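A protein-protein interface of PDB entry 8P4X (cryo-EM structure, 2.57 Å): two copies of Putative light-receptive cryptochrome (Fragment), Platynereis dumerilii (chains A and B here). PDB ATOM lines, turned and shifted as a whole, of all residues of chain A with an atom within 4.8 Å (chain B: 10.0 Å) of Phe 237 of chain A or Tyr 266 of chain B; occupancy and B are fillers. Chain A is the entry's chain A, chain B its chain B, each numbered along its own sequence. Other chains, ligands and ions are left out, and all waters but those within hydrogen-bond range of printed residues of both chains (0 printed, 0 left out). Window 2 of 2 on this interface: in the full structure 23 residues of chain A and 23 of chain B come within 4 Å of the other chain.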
ATOM      1  N   LYS A 235       3.253 -18.160   9.988  1.00  0.00           N
ATOM      2  CA  LYS A 235       2.426 -17.616  11.065  1.00  0.00           C
ATOM      3  C   LYS A 235       1.442 -16.611  10.485  1.00  0.00           C
ATOM      4  O   LYS A 235       1.628 -15.393  10.612  1.00  0.00           O
ATOM      5  CB  LYS A 235       3.295 -16.973  12.145  1.00  0.00           C
ATOM      6  CG  LYS A 235       4.127 -17.971  12.934  1.00  0.00           C
ATOM      7  CD  LYS A 235       5.230 -17.290  13.729  1.00  0.00           C
ATOM      8  CE  LYS A 235       6.536 -17.233  12.951  1.00  0.00           C
ATOM      9  NZ  LYS A 235       6.426 -16.474  11.676  1.00  0.00           N
ATOM     10  N   PRO A 236       0.380 -17.084   9.841  1.00  0.00           N
ATOM     11  CA  PRO A 236      -0.632 -16.170   9.307  1.00  0.00           C
ATOM     12  C   PRO A 236      -1.558 -15.642  10.393  1.00  0.00           C
ATOM     13  O   PRO A 236      -1.670 -16.196  11.488  1.00  0.00           O
ATOM     14  CB  PRO A 236      -1.397 -17.041   8.305  1.00  0.00           C
ATOM     15  CG  PRO A 236      -1.243 -18.420   8.821  1.00  0.00           C
ATOM     16  CD  PRO A 236       0.101 -18.485   9.485  1.00  0.00           C
ATOM     17  N   PHE A 237      -2.230 -14.537  10.061  1.00  0.00           N
ATOM     18  CA  PHE A 237      -3.156 -13.917  11.003  1.00  0.00           C
ATOM     19  C   PHE A 237      -4.395 -14.780  11.208  1.00  0.00           C
ATOM     20  O   PHE A 237      -4.828 -14.993  12.346  1.00  0.00           O
ATOM     21  CB  PHE A 237      -3.542 -12.526  10.503  1.00  0.00           C
ATOM     22  CG  PHE A 237      -4.113 -11.632  11.562  1.00  0.00           C
ATOM     23  CD1 PHE A 237      -3.284 -10.833  12.329  1.00  0.00           C
ATOM     24  CD2 PHE A 237      -5.476 -11.581  11.785  1.00  0.00           C
ATOM     25  CE1 PHE A 237      -3.805 -10.006  13.300  1.00  0.00           C
ATOM     26  CE2 PHE A 237      -6.000 -10.756  12.756  1.00  0.00           C
ATOM     27  CZ  PHE A 237      -5.164  -9.968  13.514  1.00  0.00           C
ATOM     28  N   ASN A 238      -4.977 -15.281  10.122  1.00  0.00           N
ATOM     29  CA  ASN A 238      -6.143 -16.151  10.170  1.00  0.00           C
ATOM     30  C   ASN A 238      -5.717 -17.594   9.949  1.00  0.00           C
ATOM     31  O   ASN A 238      -4.916 -17.886   9.055  1.00  0.00           O
ATOM     32  CB  ASN A 238      -7.176 -15.748   9.115  1.00  0.00           C
ATOM     33  CG  ASN A 238      -7.899 -14.467   9.466  1.00  0.00           C
ATOM     34  OD1 ASN A 238      -8.262 -14.240  10.620  1.00  0.00           O
ATOM     35  ND2 ASN A 238      -8.114 -13.620   8.471  1.00  0.00           N
ATOM     36  N   LYS A 239      -6.261 -18.494  10.763  1.00  0.00           N
ATOM     37  CA  LYS A 239      -5.906 -19.904  10.741  1.00  0.00           C
ATOM     38  C   LYS A 239      -7.054 -20.727  10.175  1.00  0.00           C
ATOM     39  O   LYS A 239      -8.223 -20.486  10.492  1.00  0.00           O
ATOM     40  CB  LYS A 239      -5.552 -20.396  12.146  1.00  0.00           C
ATOM     41  CG  LYS A 239      -4.321 -19.732  12.737  1.00  0.00           C
ATOM     42  CD  LYS A 239      -4.608 -19.118  14.095  1.00  0.00           C
ATOM     43  CE  LYS A 239      -4.823 -20.173  15.168  1.00  0.00           C
ATOM     44  NZ  LYS A 239      -3.566 -20.890  15.515  1.00  0.00           N
ATOM     45  N   VAL A 277     -12.308  -7.493   8.903  1.00  0.00           N
ATOM     46  CA  VAL A 277     -11.406  -7.564  10.045  1.00  0.00           C
ATOM     47  C   VAL A 277     -11.794  -8.652  11.029  1.00  0.00           C
ATOM     48  O   VAL A 277     -11.159  -8.768  12.087  1.00  0.00           O
ATOM     49  CB  VAL A 277     -11.309  -6.206  10.768  1.00  0.00           C
ATOM     50  CG1 VAL A 277     -10.586  -5.199   9.901  1.00  0.00           C
ATOM     51  CG2 VAL A 277     -12.686  -5.688  11.141  1.00  0.00           C
ATOM     52  N   GLY A 278     -12.810  -9.454  10.721  1.00  0.00           N
ATOM     53  CA  GLY A 278     -13.213 -10.542  11.578  1.00  0.00           C
ATOM     54  C   GLY A 278     -13.020 -11.897  10.930  1.00  0.00           C
ATOM     55  O   GLY A 278     -12.522 -12.011   9.805  1.00  0.00           O
ATOM     56  N   PRO A 279     -13.406 -12.954  11.637  1.00  0.00           N
ATOM     57  CA  PRO A 279     -13.280 -14.310  11.089  1.00  0.00           C
ATOM     58  C   PRO A 279     -14.081 -14.464   9.808  1.00  0.00           C
ATOM     59  O   PRO A 279     -15.195 -13.932   9.699  1.00  0.00           O
ATOM     60  CB  PRO A 279     -13.844 -15.196  12.212  1.00  0.00           C
ATOM     61  CG  PRO A 279     -13.688 -14.390  13.442  1.00  0.00           C
ATOM     62  CD  PRO A 279     -13.870 -12.965  13.034  1.00  0.00           C
ATOM     63  N   GLU A 381      -2.313 -16.100   3.216  1.00  0.00           N
ATOM     64  CA  GLU A 381      -3.344 -16.970   3.773  1.00  0.00           C
ATOM     65  C   GLU A 381      -3.982 -17.887   2.739  1.00  0.00           C
ATOM     66  O   GLU A 381      -4.303 -19.035   3.055  1.00  0.00           O
ATOM     67  CB  GLU A 381      -4.436 -16.127   4.438  1.00  0.00           C
ATOM     68  CG  GLU A 381      -3.956 -15.300   5.616  1.00  0.00           C
ATOM     69  CD  GLU A 381      -5.022 -14.366   6.146  1.00  0.00           C
ATOM     70  OE1 GLU A 381      -6.185 -14.482   5.708  1.00  0.00           O
ATOM     71  OE2 GLU A 381      -4.696 -13.512   6.996  1.00  0.00           O
ATOM     72  N   ARG A 464      -3.140  -3.621   8.181  1.00  0.00           N
ATOM     73  CA  ARG A 464      -2.684  -4.928   8.642  1.00  0.00           C
ATOM     74  C   ARG A 464      -1.697  -5.556   7.664  1.00  0.00           C
ATOM     75  O   ARG A 464      -0.707  -6.167   8.084  1.00  0.00           O
ATOM     76  CB  ARG A 464      -3.883  -5.850   8.858  1.00  0.00           C
ATOM     77  CG  ARG A 464      -3.534  -7.196   9.462  1.00  0.00           C
ATOM     78  CD  ARG A 464      -4.755  -8.082   9.581  1.00  0.00           C
ATOM     79  NE  ARG A 464      -5.664  -7.636  10.629  1.00  0.00           N
ATOM     80  CZ  ARG A 464      -6.872  -8.141  10.837  1.00  0.00           C
ATOM     81  NH1 ARG A 464      -7.360  -9.103  10.073  1.00  0.00           N
ATOM     82  NH2 ARG A 464      -7.609  -7.669  11.837  1.00  0.00           N
ATOM     83  N   ILE B 257     -20.594 -18.858  18.430  1.00  0.00           N
ATOM     84  CA  ILE B 257     -19.854 -17.792  17.768  1.00  0.00           C
ATOM     85  C   ILE B 257     -18.465 -17.645  18.379  1.00  0.00           C
ATOM     86  O   ILE B 257     -17.463 -17.545  17.657  1.00  0.00           O
ATOM     87  CB  ILE B 257     -20.646 -16.476  17.849  1.00  0.00           C
ATOM     88  CG1 ILE B 257     -21.854 -16.528  16.916  1.00  0.00           C
ATOM     89  CG2 ILE B 257     -19.746 -15.300  17.510  1.00  0.00           C
ATOM     90  CD1 ILE B 257     -22.826 -15.382  17.094  1.00  0.00           C
ATOM     91  N   GLU B 258     -18.381 -17.627  19.710  1.00  0.00           N
ATOM     92  CA  GLU B 258     -17.092 -17.505  20.378  1.00  0.00           C
ATOM     93  C   GLU B 258     -16.196 -18.703  20.096  1.00  0.00           C
ATOM     94  O   GLU B 258     -14.984 -18.546  19.939  1.00  0.00           O
ATOM     95  CB  GLU B 258     -17.297 -17.343  21.886  1.00  0.00           C
ATOM     96  CG  GLU B 258     -18.038 -16.084  22.292  1.00  0.00           C
ATOM     97  CD  GLU B 258     -17.197 -14.832  22.137  1.00  0.00           C
ATOM     98  OE1 GLU B 258     -16.122 -14.908  21.508  1.00  0.00           O
ATOM     99  OE2 GLU B 258     -17.610 -13.771  22.651  1.00  0.00           O
ATOM    100  N   ARG B 259     -16.767 -19.907  20.049  1.00  0.00           N
ATOM    101  CA  ARG B 259     -15.970 -21.089  19.731  1.00  0.00           C
ATOM    102  C   ARG B 259     -15.340 -20.967  18.348  1.00  0.00           C
ATOM    103  O   ARG B 259     -14.140 -21.223  18.167  1.00  0.00           O
ATOM    104  CB  ARG B 259     -16.846 -22.339  19.822  1.00  0.00           C
ATOM    105  CG  ARG B 259     -16.191 -23.612  19.328  1.00  0.00           C
ATOM    106  CD  ARG B 259     -17.141 -24.786  19.442  1.00  0.00           C
ATOM    107  NE  ARG B 259     -17.324 -25.212  20.825  1.00  0.00           N
ATOM    108  CZ  ARG B 259     -16.734 -26.261  21.382  1.00  0.00           C
ATOM    109  NH1 ARG B 259     -15.916 -27.045  20.697  1.00  0.00           N
ATOM    110  NH2 ARG B 259     -16.973 -26.536  22.660  1.00  0.00           N
ATOM    111  N   THR B 260     -16.142 -20.576  17.356  1.00  0.00           N
ATOM    112  CA  THR B 260     -15.607 -20.401  16.011  1.00  0.00           C
ATOM    113  C   THR B 260     -14.538 -19.314  15.971  1.00  0.00           C
ATOM    114  O   THR B 260     -13.500 -19.491  15.321  1.00  0.00           O
ATOM    115  CB  THR B 260     -16.745 -20.087  15.040  1.00  0.00           C
ATOM    116  OG1 THR B 260     -17.624 -21.215  14.957  1.00  0.00           O
ATOM    117  CG2 THR B 260     -16.207 -19.775  13.661  1.00  0.00           C
ATOM    118  N   ALA B 261     -14.760 -18.196  16.667  1.00  0.00           N
ATOM    119  CA  ALA B 261     -13.749 -17.144  16.717  1.00  0.00           C
ATOM    120  C   ALA B 261     -12.452 -17.633  17.357  1.00  0.00           C
ATOM    121  O   ALA B 261     -11.362 -17.312  16.874  1.00  0.00           O
ATOM    122  CB  ALA B 261     -14.290 -15.931  17.471  1.00  0.00           C
ATOM    123  N   TYR B 262     -12.548 -18.400  18.446  1.00  0.00           N
ATOM    124  CA  TYR B 262     -11.347 -18.952  19.068  1.00  0.00           C
ATOM    125  C   TYR B 262     -10.596 -19.847  18.096  1.00  0.00           C
ATOM    126  O   TYR B 262      -9.365 -19.779  18.001  1.00  0.00           O
ATOM    127  CB  TYR B 262     -11.706 -19.744  20.329  1.00  0.00           C
ATOM    128  CG  TYR B 262     -12.416 -18.960  21.410  1.00  0.00           C
ATOM    129  CD1 TYR B 262     -12.258 -17.588  21.527  1.00  0.00           C
ATOM    130  CD2 TYR B 262     -13.243 -19.602  22.321  1.00  0.00           C
ATOM    131  CE1 TYR B 262     -12.906 -16.879  22.515  1.00  0.00           C
ATOM    132  CE2 TYR B 262     -13.893 -18.902  23.309  1.00  0.00           C
ATOM    133  CZ  TYR B 262     -13.723 -17.542  23.403  1.00  0.00           C
ATOM    134  OH  TYR B 262     -14.373 -16.844  24.392  1.00  0.00           O
ATOM    135  N   LYS B 263     -11.318 -20.704  17.371  1.00  0.00           N
ATOM    136  CA  LYS B 263     -10.658 -21.558  16.389  1.00  0.00           C
ATOM    137  C   LYS B 263      -9.964 -20.730  15.314  1.00  0.00           C
ATOM    138  O   LYS B 263      -8.862 -21.074  14.871  1.00  0.00           O
ATOM    139  CB  LYS B 263     -11.663 -22.520  15.761  1.00  0.00           C
ATOM    140  CG  LYS B 263     -11.936 -23.749  16.599  1.00  0.00           C
ATOM    141  CD  LYS B 263     -12.793 -24.746  15.849  1.00  0.00           C
ATOM    142  CE  LYS B 263     -12.978 -26.026  16.642  1.00  0.00           C
ATOM    143  NZ  LYS B 263     -13.815 -25.817  17.850  1.00  0.00           N
ATOM    144  N   ALA B 264     -10.593 -19.637  14.878  1.00  0.00           N
ATOM    145  CA  ALA B 264      -9.974 -18.779  13.873  1.00  0.00           C
ATOM    146  C   ALA B 264      -8.717 -18.087  14.387  1.00  0.00           C
ATOM    147  O   ALA B 264      -7.808 -17.818  13.595  1.00  0.00           O
ATOM    148  CB  ALA B 264     -10.973 -17.733  13.383  1.00  0.00           C
ATOM    149  N   GLY B 265      -8.646 -17.786  15.678  1.00  0.00           N
ATOM    150  CA  GLY B 265      -7.487 -17.153  16.262  1.00  0.00           C
ATOM    151  C   GLY B 265      -7.733 -15.808  16.909  1.00  0.00           C
ATOM    152  O   GLY B 265      -6.812 -14.985  16.947  1.00  0.00           O
ATOM    153  N   TYR B 266      -8.936 -15.558  17.419  1.00  0.00           N
ATOM    154  CA  TYR B 266      -9.308 -14.281  18.025  1.00  0.00           C
ATOM    155  C   TYR B 266      -9.661 -14.526  19.492  1.00  0.00           C
ATOM    156  O   TYR B 266     -10.776 -14.945  19.811  1.00  0.00           O
ATOM    157  CB  TYR B 266     -10.476 -13.643  17.267  1.00  0.00           C
ATOM    158  CG  TYR B 266     -10.153 -13.243  15.846  1.00  0.00           C
ATOM    159  CD1 TYR B 266      -9.977 -14.200  14.859  1.00  0.00           C
ATOM    160  CD2 TYR B 266     -10.038 -11.909  15.490  1.00  0.00           C
ATOM    161  CE1 TYR B 266      -9.683 -13.840  13.560  1.00  0.00           C
ATOM    162  CE2 TYR B 266      -9.746 -11.540  14.193  1.00  0.00           C
ATOM    163  CZ  TYR B 266      -9.570 -12.509  13.234  1.00  0.00           C
ATOM    164  OH  TYR B 266      -9.280 -12.148  11.940  1.00  0.00           O
ATOM    165  N   ILE B 267      -8.709 -14.259  20.381  1.00  0.00           N
ATOM    166  CA  ILE B 267      -8.898 -14.391  21.822  1.00  0.00           C
ATOM    167  C   ILE B 267      -8.807 -12.995  22.424  1.00  0.00           C
ATOM    168  O   ILE B 267      -7.739 -12.371  22.411  1.00  0.00           O
ATOM    169  CB  ILE B 267      -7.868 -15.338  22.456  1.00  0.00           C
ATOM    170  CG1 ILE B 267      -8.166 -16.795  22.091  1.00  0.00           C
ATOM    171  CG2 ILE B 267      -7.857 -15.187  23.967  1.00  0.00           C
ATOM    172  CD1 ILE B 267      -7.793 -17.169  20.690  1.00  0.00           C
ATOM    173  N   MET B 268      -9.928 -12.510  22.961  1.00  0.00           N
ATOM    174  CA  MET B 268     -10.032 -11.183  23.560  1.00  0.00           C
ATOM    175  C   MET B 268      -9.346 -10.135  22.690  1.00  0.00           C
ATOM    176  O   MET B 268      -8.277  -9.630  23.056  1.00  0.00           O
ATOM    177  CB  MET B 268      -9.424 -11.172  24.965  1.00  0.00           C
ATOM    178  CG  MET B 268     -10.078 -12.138  25.942  1.00  0.00           C
ATOM    179  SD  MET B 268     -11.851 -11.879  26.134  1.00  0.00           S
ATOM    180  CE  MET B 268     -11.889 -10.179  26.689  1.00  0.00           C
ATOM    181  N   PRO B 269      -9.919  -9.784  21.544  1.00  0.00           N
ATOM    182  CA  PRO B 269      -9.335  -8.741  20.702  1.00  0.00           C
ATOM    183  C   PRO B 269      -9.905  -7.364  21.024  1.00  0.00           C
ATOM    184  O   PRO B 269     -10.927  -7.222  21.699  1.00  0.00           O
ATOM    185  CB  PRO B 269      -9.727  -9.185  19.286  1.00  0.00           C
ATOM    186  CG  PRO B 269     -10.939 -10.071  19.464  1.00  0.00           C
ATOM    187  CD  PRO B 269     -11.135 -10.342  20.934  1.00  0.00           C
ATOM    188  N   ASN B 270      -9.216  -6.343  20.522  1.00  0.00           N
ATOM    189  CA  ASN B 270      -9.660  -4.970  20.726  1.00  0.00           C
ATOM    190  C   ASN B 270     -10.954  -4.708  19.968  1.00  0.00           C
ATOM    191  O   ASN B 270     -11.118  -5.127  18.819  1.00  0.00           O
ATOM    192  CB  ASN B 270      -8.582  -3.987  20.275  1.00  0.00           C
ATOM    193  CG  ASN B 270      -7.351  -4.024  21.156  1.00  0.00           C
ATOM    194  OD1 ASN B 270      -7.426  -4.367  22.336  1.00  0.00           O
ATOM    195  ND2 ASN B 270      -6.207  -3.667  20.587  1.00  0.00           N
ATOM    196  N   GLN B 271     -11.875  -4.003  20.619  1.00  0.00           N
ATOM    197  CA  GLN B 271     -13.181  -3.677  20.057  1.00  0.00           C
ATOM    198  C   GLN B 271     -13.188  -2.207  19.655  1.00  0.00           C
ATOM    199  O   GLN B 271     -13.128  -1.323  20.516  1.00  0.00           O
ATOM    200  CB  GLN B 271     -14.292  -3.973  21.060  1.00  0.00           C
ATOM    201  CG  GLN B 271     -14.656  -5.441  21.175  1.00  0.00           C
ATOM    202  CD  GLN B 271     -15.846  -5.673  22.080  1.00  0.00           C
ATOM    203  OE1 GLN B 271     -15.929  -5.110  23.171  1.00  0.00           O
ATOM    204  NE2 GLN B 271     -16.781  -6.496  21.627  1.00  0.00           N
ATOM    205  N   ASN B 304     -16.816 -23.435  27.811  1.00  0.00           N
ATOM    206  CA  ASN B 304     -16.652 -23.357  26.365  1.00  0.00           C
ATOM    207  C   ASN B 304     -15.215 -23.019  25.996  1.00  0.00           C
ATOM    208  O   ASN B 304     -14.646 -23.616  25.075  1.00  0.00           O
ATOM    209  CB  ASN B 304     -17.615 -22.318  25.790  1.00  0.00           C
ATOM    210  CG  ASN B 304     -17.532 -22.208  24.284  1.00  0.00           C
ATOM    211  OD1 ASN B 304     -16.783 -21.394  23.749  1.00  0.00           O
ATOM    212  ND2 ASN B 304     -18.311 -23.024  23.592  1.00  0.00           N
ATOM    213  N   TYR B 305     -14.608 -22.064  26.705  1.00  0.00           N
ATOM    214  CA  TYR B 305     -13.214 -21.732  26.424  1.00  0.00           C
ATOM    215  C   TYR B 305     -12.295 -22.919  26.689  1.00  0.00           C
ATOM    216  O   TYR B 305     -11.397 -23.208  25.890  1.00  0.00           O
ATOM    217  CB  TYR B 305     -12.780 -20.530  27.260  1.00  0.00           C
ATOM    218  CG  TYR B 305     -11.301 -20.231  27.163  1.00  0.00           C
ATOM    219  CD1 TYR B 305     -10.785 -19.521  26.090  1.00  0.00           C
ATOM    220  CD2 TYR B 305     -10.422 -20.659  28.148  1.00  0.00           C
ATOM    221  CE1 TYR B 305      -9.438 -19.249  25.999  1.00  0.00           C
ATOM    222  CE2 TYR B 305      -9.075 -20.391  28.065  1.00  0.00           C
ATOM    223  CZ  TYR B 305      -8.587 -19.685  26.990  1.00  0.00           C
ATOM    224  OH  TYR B 305      -7.242 -19.413  26.903  1.00  0.00           O
ATOM    225  N   VAL B 308     -12.194 -25.942  23.997  1.00  0.00           N
ATOM    226  CA  VAL B 308     -11.440 -25.723  22.765  1.00  0.00           C
ATOM    227  C   VAL B 308      -9.953 -25.585  23.063  1.00  0.00           C
ATOM    228  O   VAL B 308      -9.130 -26.381  22.597  1.00  0.00           O
ATOM    229  CB  VAL B 308     -11.974 -24.486  22.020  1.00  0.00           C
ATOM    230  CG1 VAL B 308     -11.248 -24.306  20.700  1.00  0.00           C
ATOM    231  CG2 VAL B 308     -13.467 -24.600  21.792  1.00  0.00           C
ATOM    232  N   CYS B 309      -9.590 -24.573  23.842  1.00  0.00           N
ATOM    233  CA  CYS B 309      -8.200 -24.293  24.160  1.00  0.00           C
ATOM    234  C   CYS B 309      -7.777 -25.113  25.379  1.00  0.00           C
ATOM    235  O   CYS B 309      -8.465 -26.046  25.798  1.00  0.00           O
ATOM    236  CB  CYS B 309      -8.007 -22.795  24.379  1.00  0.00           C
ATOM    237  SG  CYS B 309      -8.633 -21.771  23.029  1.00  0.00           S
ATOM    238  N   LEU B 314      -8.566 -17.907  32.415  1.00  0.00           N
ATOM    239  CA  LEU B 314      -8.492 -16.580  31.805  1.00  0.00           C
ATOM    240  C   LEU B 314      -9.696 -15.778  32.291  1.00  0.00           C
ATOM    241  O   LEU B 314     -10.818 -15.980  31.817  1.00  0.00           O
ATOM    242  CB  LEU B 314      -8.462 -16.678  30.284  1.00  0.00           C
ATOM    243  CG  LEU B 314      -8.325 -15.361  29.522  1.00  0.00           C
ATOM    244  CD1 LEU B 314      -7.008 -14.683  29.848  1.00  0.00           C
ATOM    245  CD2 LEU B 314      -8.452 -15.606  28.035  1.00  0.00           C
ATOM    246  N   LEU B 317     -12.563 -13.187  30.255  1.00  0.00           N
ATOM    247  CA  LEU B 317     -13.762 -13.582  29.523  1.00  0.00           C
ATOM    248  C   LEU B 317     -15.017 -12.997  30.156  1.00  0.00           C
ATOM    249  O   LEU B 317     -15.921 -12.535  29.449  1.00  0.00           O
ATOM    250  CB  LEU B 317     -13.859 -15.106  29.464  1.00  0.00           C
ATOM    251  CG  LEU B 317     -12.703 -15.850  28.797  1.00  0.00           C
ATOM    252  CD1 LEU B 317     -12.886 -17.339  28.971  1.00  0.00           C
ATOM    253  CD2 LEU B 317     -12.594 -15.498  27.325  1.00  0.00           C
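OH of Tyr 266 of chain B sits at hydrogen-bond distance from OD1 of Asn 238 of chain A, 2.7 Å away. N of Lys 239 of chain A sits at hydrogen-bond distance from O of Ala 264 of chain B (3.3 Å).
N of Tyr 266 of chain B is in hydrogen-bond range of O of Ala 261 of chain B. The side-chain amide nitrogen (ND2) of Asn 238 of chain A lies within hydrogen-bond range of the side-chain carboxylate (OE1) of Glu 381 of chain A (3.5 Å).
Among the printed residues, pairs that only touch across the chains: Phe 237 of chain A with Tyr 266 of chain B (3.7 Å), Val 277 of chain A with Tyr 266 of chain B (3.8 Å), Gly 278 of chain A with Tyr 266 of chain B (3.9 Å) and Pro 279 of chain A with Tyr 266 of chain B (3.98 Å).
Phe 237 of chain A touches one residue of chain B. Of the printed residues of chain A, Tyr 266 of chain B touches Phe 237 (3.7 Å), Asn 238 (2.7 Å), Val 277 (3.8 Å), Gly 278 (3.9 Å) and Pro 279 (3.98 Å). Pro 236 of chain A touches none of the printed residues of chain B. Of the printed residues of chain B, Gly 278 of chain A touches Tyr 266. Of the printed residues of chain A, Ala 264 of chain B touches Lys 239 (3.3 Å). Printed residues of chain B within 4 Å of Val 277 of chain A: Tyr 266 (3.8 Å). Met 268 of chain B touches none of the printed residues of chain A. Ile 267 of chain B touches none of the printed residues of chain A. The nearest printed residue of chain B that does not touch Pro 279 of chain A is Ala 264 of chain B (4.01 Å).
Hydrophobic or aromatic side chains of chain A within 4 Å of the printed part of chain B: Phe 237 and Pro 279. Hydrophobic or aromatic side chains of chain B within 4 Å of the printed part of chain A: Tyr 266. Among the printed residues, 6 pairs touch across the chains. Among the printed residues, no Asp or Glu carboxylate lies within 4 Å of a Lys or Arg side-chain nitrogen of the other chain.
No position is printed for both chains.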
